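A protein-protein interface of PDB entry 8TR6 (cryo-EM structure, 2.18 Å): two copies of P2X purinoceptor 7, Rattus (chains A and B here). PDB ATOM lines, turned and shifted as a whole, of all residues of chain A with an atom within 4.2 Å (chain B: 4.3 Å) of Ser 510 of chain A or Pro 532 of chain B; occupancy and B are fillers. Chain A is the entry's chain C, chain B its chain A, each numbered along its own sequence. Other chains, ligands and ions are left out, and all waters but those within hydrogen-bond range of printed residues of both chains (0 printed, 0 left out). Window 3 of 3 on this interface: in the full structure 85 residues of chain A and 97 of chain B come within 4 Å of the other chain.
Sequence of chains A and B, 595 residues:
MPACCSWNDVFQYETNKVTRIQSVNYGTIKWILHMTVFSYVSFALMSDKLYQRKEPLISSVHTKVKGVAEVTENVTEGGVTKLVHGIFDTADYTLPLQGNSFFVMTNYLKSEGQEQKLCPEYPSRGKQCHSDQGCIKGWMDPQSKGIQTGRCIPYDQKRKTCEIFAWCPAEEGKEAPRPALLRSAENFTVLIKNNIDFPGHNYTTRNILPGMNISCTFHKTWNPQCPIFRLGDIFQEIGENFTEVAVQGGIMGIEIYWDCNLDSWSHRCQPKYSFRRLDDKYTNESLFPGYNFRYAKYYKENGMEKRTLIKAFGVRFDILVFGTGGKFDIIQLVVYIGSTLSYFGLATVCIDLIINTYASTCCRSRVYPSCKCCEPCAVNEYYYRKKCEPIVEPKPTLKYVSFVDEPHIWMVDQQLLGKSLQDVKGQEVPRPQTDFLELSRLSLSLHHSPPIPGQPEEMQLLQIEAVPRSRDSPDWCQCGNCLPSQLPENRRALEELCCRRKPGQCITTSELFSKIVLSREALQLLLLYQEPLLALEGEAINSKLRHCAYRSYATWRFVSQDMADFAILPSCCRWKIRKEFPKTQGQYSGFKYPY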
ATOM      1  N   ILE A 507      18.064 -25.680 -24.933  1.00  0.00           N
ATOM      2  CA  ILE A 507      17.078 -25.630 -23.858  1.00  0.00           C
ATOM      3  C   ILE A 507      16.324 -24.309 -23.883  1.00  0.00           C
ATOM      4  O   ILE A 507      15.173 -24.233 -23.439  1.00  0.00           O
ATOM      5  CB  ILE A 507      17.766 -25.860 -22.499  1.00  0.00           C
ATOM      6  CG1 ILE A 507      16.718 -26.062 -21.404  1.00  0.00           C
ATOM      7  CG2 ILE A 507      18.673 -24.692 -22.159  1.00  0.00           C
ATOM      8  CD1 ILE A 507      17.307 -26.335 -20.048  1.00  0.00           C
ATOM      9  N   THR A 508      16.955 -23.251 -24.395  1.00  0.00           N
ATOM     10  CA  THR A 508      16.289 -21.954 -24.459  1.00  0.00           C
ATOM     11  C   THR A 508      15.063 -21.995 -25.362  1.00  0.00           C
ATOM     12  O   THR A 508      14.128 -21.209 -25.173  1.00  0.00           O
ATOM     13  CB  THR A 508      17.262 -20.882 -24.951  1.00  0.00           C
ATOM     14  OG1 THR A 508      17.730 -21.221 -26.263  1.00  0.00           O
ATOM     15  CG2 THR A 508      18.449 -20.756 -24.008  1.00  0.00           C
ATOM     16  N   THR A 509      15.049 -22.897 -26.345  1.00  0.00           N
ATOM     17  CA  THR A 509      13.920 -22.976 -27.264  1.00  0.00           C
ATOM     18  C   THR A 509      12.636 -23.399 -26.566  1.00  0.00           C
ATOM     19  O   THR A 509      11.546 -23.109 -27.070  1.00  0.00           O
ATOM     20  CB  THR A 509      14.237 -23.950 -28.399  1.00  0.00           C
ATOM     21  OG1 THR A 509      14.532 -25.242 -27.857  1.00  0.00           O
ATOM     22  CG2 THR A 509      15.426 -23.455 -29.208  1.00  0.00           C
ATOM     23  N   SER A 510      12.736 -24.077 -25.427  1.00  0.00           N
ATOM     24  CA  SER A 510      11.549 -24.498 -24.701  1.00  0.00           C
ATOM     25  C   SER A 510      10.793 -23.287 -24.167  1.00  0.00           C
ATOM     26  O   SER A 510      11.393 -22.327 -23.676  1.00  0.00           O
ATOM     27  CB  SER A 510      11.934 -25.427 -23.551  1.00  0.00           C
ATOM     28  OG  SER A 510      12.548 -24.705 -22.498  1.00  0.00           O
ATOM     29  N   GLU A 511       9.463 -23.338 -24.268  1.00  0.00           N
ATOM     30  CA  GLU A 511       8.647 -22.235 -23.772  1.00  0.00           C
ATOM     31  C   GLU A 511       8.763 -22.097 -22.261  1.00  0.00           C
ATOM     32  O   GLU A 511       8.646 -20.987 -21.726  1.00  0.00           O
ATOM     33  CB  GLU A 511       7.186 -22.440 -24.174  1.00  0.00           C
ATOM     34  N   LEU A 512       8.987 -23.208 -21.556  1.00  0.00           N
ATOM     35  CA  LEU A 512       9.131 -23.137 -20.108  1.00  0.00           C
ATOM     36  C   LEU A 512      10.349 -22.316 -19.716  1.00  0.00           C
ATOM     37  O   LEU A 512      10.360 -21.690 -18.651  1.00  0.00           O
ATOM     38  CB  LEU A 512       9.222 -24.544 -19.518  1.00  0.00           C
ATOM     39  CG  LEU A 512       8.624 -24.687 -18.118  1.00  0.00           C
ATOM     40  CD1 LEU A 512       7.122 -24.902 -18.211  1.00  0.00           C
ATOM     41  CD2 LEU A 512       9.282 -25.820 -17.356  1.00  0.00           C
ATOM     42  N   PHE A 513      11.386 -22.305 -20.558  1.00  0.00           N
ATOM     43  CA  PHE A 513      12.542 -21.457 -20.292  1.00  0.00           C
ATOM     44  C   PHE A 513      12.139 -19.990 -20.272  1.00  0.00           C
ATOM     45  O   PHE A 513      12.537 -19.234 -19.378  1.00  0.00           O
ATOM     46  CB  PHE A 513      13.624 -21.703 -21.345  1.00  0.00           C
ATOM     47  CG  PHE A 513      14.877 -20.908 -21.128  1.00  0.00           C
ATOM     48  CD1 PHE A 513      14.988 -19.614 -21.609  1.00  0.00           C
ATOM     49  CD2 PHE A 513      15.948 -21.454 -20.444  1.00  0.00           C
ATOM     50  CE1 PHE A 513      16.140 -18.885 -21.408  1.00  0.00           C
ATOM     51  CE2 PHE A 513      17.099 -20.727 -20.242  1.00  0.00           C
ATOM     52  CZ  PHE A 513      17.196 -19.441 -20.725  1.00  0.00           C
ATOM     53  N   SER A 514      11.342 -19.570 -21.256  1.00  0.00           N
ATOM     54  CA  SER A 514      10.864 -18.192 -21.281  1.00  0.00           C
ATOM     55  C   SER A 514       9.940 -17.909 -20.104  1.00  0.00           C
ATOM     56  O   SER A 514      10.009 -16.833 -19.498  1.00  0.00           O
ATOM     57  CB  SER A 514      10.149 -17.913 -22.603  1.00  0.00           C
ATOM     58  OG  SER A 514       8.932 -18.634 -22.683  1.00  0.00           O
ATOM     59  N   TRP A 556      15.762 -24.044 -11.065  1.00  0.00           N
ATOM     60  CA  TRP A 556      14.977 -24.952 -11.890  1.00  0.00           C
ATOM     61  C   TRP A 556      15.791 -26.168 -12.315  1.00  0.00           C
ATOM     62  O   TRP A 556      15.296 -27.298 -12.273  1.00  0.00           O
ATOM     63  CB  TRP A 556      14.446 -24.192 -13.105  1.00  0.00           C
ATOM     64  CG  TRP A 556      13.919 -25.043 -14.219  1.00  0.00           C
ATOM     65  CD1 TRP A 556      13.253 -26.229 -14.110  1.00  0.00           C
ATOM     66  CD2 TRP A 556      14.008 -24.763 -15.619  1.00  0.00           C
ATOM     67  NE1 TRP A 556      12.926 -26.704 -15.355  1.00  0.00           N
ATOM     68  CE2 TRP A 556      13.378 -25.822 -16.299  1.00  0.00           C
ATOM     69  CE3 TRP A 556      14.560 -23.719 -16.365  1.00  0.00           C
ATOM     70  CZ2 TRP A 556      13.286 -25.866 -17.687  1.00  0.00           C
ATOM     71  CZ3 TRP A 556      14.468 -23.766 -17.742  1.00  0.00           C
ATOM     72  CH2 TRP A 556      13.836 -24.831 -18.387  1.00  0.00           C
ATOM     73  N   ARG A 557      17.043 -25.961 -12.720  1.00  0.00           N
ATOM     74  CA  ARG A 557      17.854 -27.052 -13.244  1.00  0.00           C
ATOM     75  C   ARG A 557      18.701 -27.749 -12.186  1.00  0.00           C
ATOM     76  O   ARG A 557      19.315 -28.776 -12.491  1.00  0.00           O
ATOM     77  CB  ARG A 557      18.759 -26.533 -14.364  1.00  0.00           C
ATOM     78  CG  ARG A 557      17.998 -25.912 -15.520  1.00  0.00           C
ATOM     79  CD  ARG A 557      17.726 -26.913 -16.619  1.00  0.00           C
ATOM     80  NE  ARG A 557      16.865 -28.001 -16.166  1.00  0.00           N
ATOM     81  CZ  ARG A 557      17.072 -29.288 -16.409  1.00  0.00           C
ATOM     82  NH1 ARG A 557      18.114 -29.707 -17.111  1.00  0.00           N
ATOM     83  NH2 ARG A 557      16.210 -30.183 -15.936  1.00  0.00           N
ATOM     84  N   LEU B 528       7.500 -30.699 -18.146  1.00  0.00           N
ATOM     85  CA  LEU B 528       8.548 -29.875 -18.738  1.00  0.00           C
ATOM     86  C   LEU B 528       9.534 -29.403 -17.679  1.00  0.00           C
ATOM     87  O   LEU B 528      10.745 -29.357 -17.922  1.00  0.00           O
ATOM     88  CB  LEU B 528       7.929 -28.687 -19.471  1.00  0.00           C
ATOM     89  CG  LEU B 528       7.099 -29.044 -20.705  1.00  0.00           C
ATOM     90  CD1 LEU B 528       6.346 -27.830 -21.211  1.00  0.00           C
ATOM     91  CD2 LEU B 528       7.974 -29.628 -21.800  1.00  0.00           C
ATOM     92  N   GLN B 530      10.545 -30.913 -15.080  1.00  0.00           N
ATOM     93  CA  GLN B 530      11.494 -31.991 -14.870  1.00  0.00           C
ATOM     94  C   GLN B 530      12.233 -32.309 -16.157  1.00  0.00           C
ATOM     95  O   GLN B 530      13.449 -32.487 -16.144  1.00  0.00           O
ATOM     96  CB  GLN B 530      10.765 -33.231 -14.375  1.00  0.00           C
ATOM     97  CG  GLN B 530      11.671 -34.429 -14.165  1.00  0.00           C
ATOM     98  CD  GLN B 530      10.949 -35.599 -13.530  1.00  0.00           C
ATOM     99  OE1 GLN B 530       9.735 -35.560 -13.329  1.00  0.00           O
ATOM    100  NE2 GLN B 530      11.693 -36.649 -13.213  1.00  0.00           N
ATOM    101  N   GLU B 531      11.504 -32.388 -17.265  1.00  0.00           N
ATOM    102  CA  GLU B 531      12.106 -32.705 -18.558  1.00  0.00           C
ATOM    103  C   GLU B 531      11.803 -31.585 -19.533  1.00  0.00           C
ATOM    104  O   GLU B 531      10.794 -31.627 -20.231  1.00  0.00           O
ATOM    105  CB  GLU B 531      11.561 -34.031 -19.080  1.00  0.00           C
ATOM    106  CG  GLU B 531      11.445 -35.116 -18.020  1.00  0.00           C
ATOM    107  CD  GLU B 531      10.044 -35.251 -17.452  1.00  0.00           C
ATOM    108  OE1 GLU B 531       9.063 -35.020 -18.190  1.00  0.00           O
ATOM    109  OE2 GLU B 531       9.920 -35.619 -16.266  1.00  0.00           O
ATOM    110  N   PRO B 532      12.681 -30.576 -19.601  1.00  0.00           N
ATOM    111  CA  PRO B 532      12.366 -29.409 -20.445  1.00  0.00           C
ATOM    112  C   PRO B 532      12.096 -29.749 -21.901  1.00  0.00           C
ATOM    113  O   PRO B 532      11.232 -29.121 -22.523  1.00  0.00           O
ATOM    114  CB  PRO B 532      13.613 -28.526 -20.294  1.00  0.00           C
ATOM    115  CG  PRO B 532      14.262 -28.974 -19.037  1.00  0.00           C
ATOM    116  CD  PRO B 532      13.979 -30.432 -18.921  1.00  0.00           C
ATOM    117  N   LEU B 533      12.808 -30.724 -22.465  1.00  0.00           N
ATOM    118  CA  LEU B 533      12.686 -31.065 -23.876  1.00  0.00           C
ATOM    119  C   LEU B 533      11.790 -32.275 -24.113  1.00  0.00           C
ATOM    120  O   LEU B 533      11.860 -32.889 -25.182  1.00  0.00           O
ATOM    121  CB  LEU B 533      14.068 -31.313 -24.476  1.00  0.00           C
ATOM    122  CG  LEU B 533      15.066 -30.167 -24.309  1.00  0.00           C
ATOM    123  CD1 LEU B 533      16.404 -30.540 -24.916  1.00  0.00           C
ATOM    124  CD2 LEU B 533      14.530 -28.889 -24.930  1.00  0.00           C
ATOM    125  N   LEU B 534      10.952 -32.628 -23.142  1.00  0.00           N
ATOM    126  CA  LEU B 534      10.047 -33.755 -23.313  1.00  0.00           C
ATOM    127  C   LEU B 534       9.139 -33.524 -24.514  1.00  0.00           C
ATOM    128  O   LEU B 534       8.588 -32.434 -24.692  1.00  0.00           O
ATOM    129  CB  LEU B 534       9.214 -33.952 -22.050  1.00  0.00           C
ATOM    130  CG  LEU B 534       8.395 -35.240 -21.979  1.00  0.00           C
ATOM    131  CD1 LEU B 534       9.275 -36.411 -21.576  1.00  0.00           C
ATOM    132  CD2 LEU B 534       7.240 -35.070 -21.008  1.00  0.00           C
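Pro 532 of chain B touches Ser 510 of chain A (O to CB, 3.9 Å). C of Leu 528 of chain B touches CD2 of Leu 512 of chain A, 3.6 Å away. Pro 532 of chain B touches Trp 556 of chain A. NH2 of Arg 557 of chain A touches O of Gln 530 of chain B, at 3.6 Å. Pro 532 of chain B touches Arg 557 of chain A (CD to NH2, 3.7 Å).
Hydrophobic or aromatic side chains of chain A that line the printed part of chain B: Leu 512 and Trp 556. Along chain A the printed residues that touch a printed residue of chain B span positions 510 to 557. Among the printed residues, no Asp or Glu carboxylate lies within 4 Å of a Lys or Arg side-chain nitrogen of the other chain.
The side-chain amide oxygen of Gln 530 of chain B sits close to the side-chain carboxylate of Glu 531 of chain B (2.9 Å). The backbone carbonyl oxygen (O) of Ile 507 of chain A is in hydrogen-bond range of the side-chain hydroxyl (OG) of Ser 510 of chain A (2.8 Å). OG of Ser 510 of chain A is in hydrogen-bond range of N of Phe 513 of chain A (3.3 Å).
Thr 509 of chain A touches none of the printed residues of chain B. Of the printed residues of chain B, Leu 512 of chain A touches Leu 528. Printed residues of chain B within 4 Å of Trp 556 of chain A: Pro 532. Of the printed residues of chain B, Arg 557 of chain A touches Gln 530 (3.6 Å) and Pro 532 (3.7 Å). Of the printed residues of chain A, Leu 528 of chain B touches Leu 512 (3.6 Å). Printed residues of chain A within 4 Å of Gln 530 of chain B: Arg 557. Pro 532 of chain B touches just these residues of chain A: Ser 510 (3.9 Å), Trp 556 (3.5 Å) and Arg 557 (3.7 Å). The nearest printed residue of chain B that does not touch Ser 510 of chain A is Leu 533 of chain B (4.5 Å). The nearest residue of chain A that does not touch Pro 532 of chain B is Ile 507 of chain A (4.1 Å).
No position is printed for both chains. Of the 5 pairs that touch across the chains among the printed residues, none has its exchanged pair printed and touching as well.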
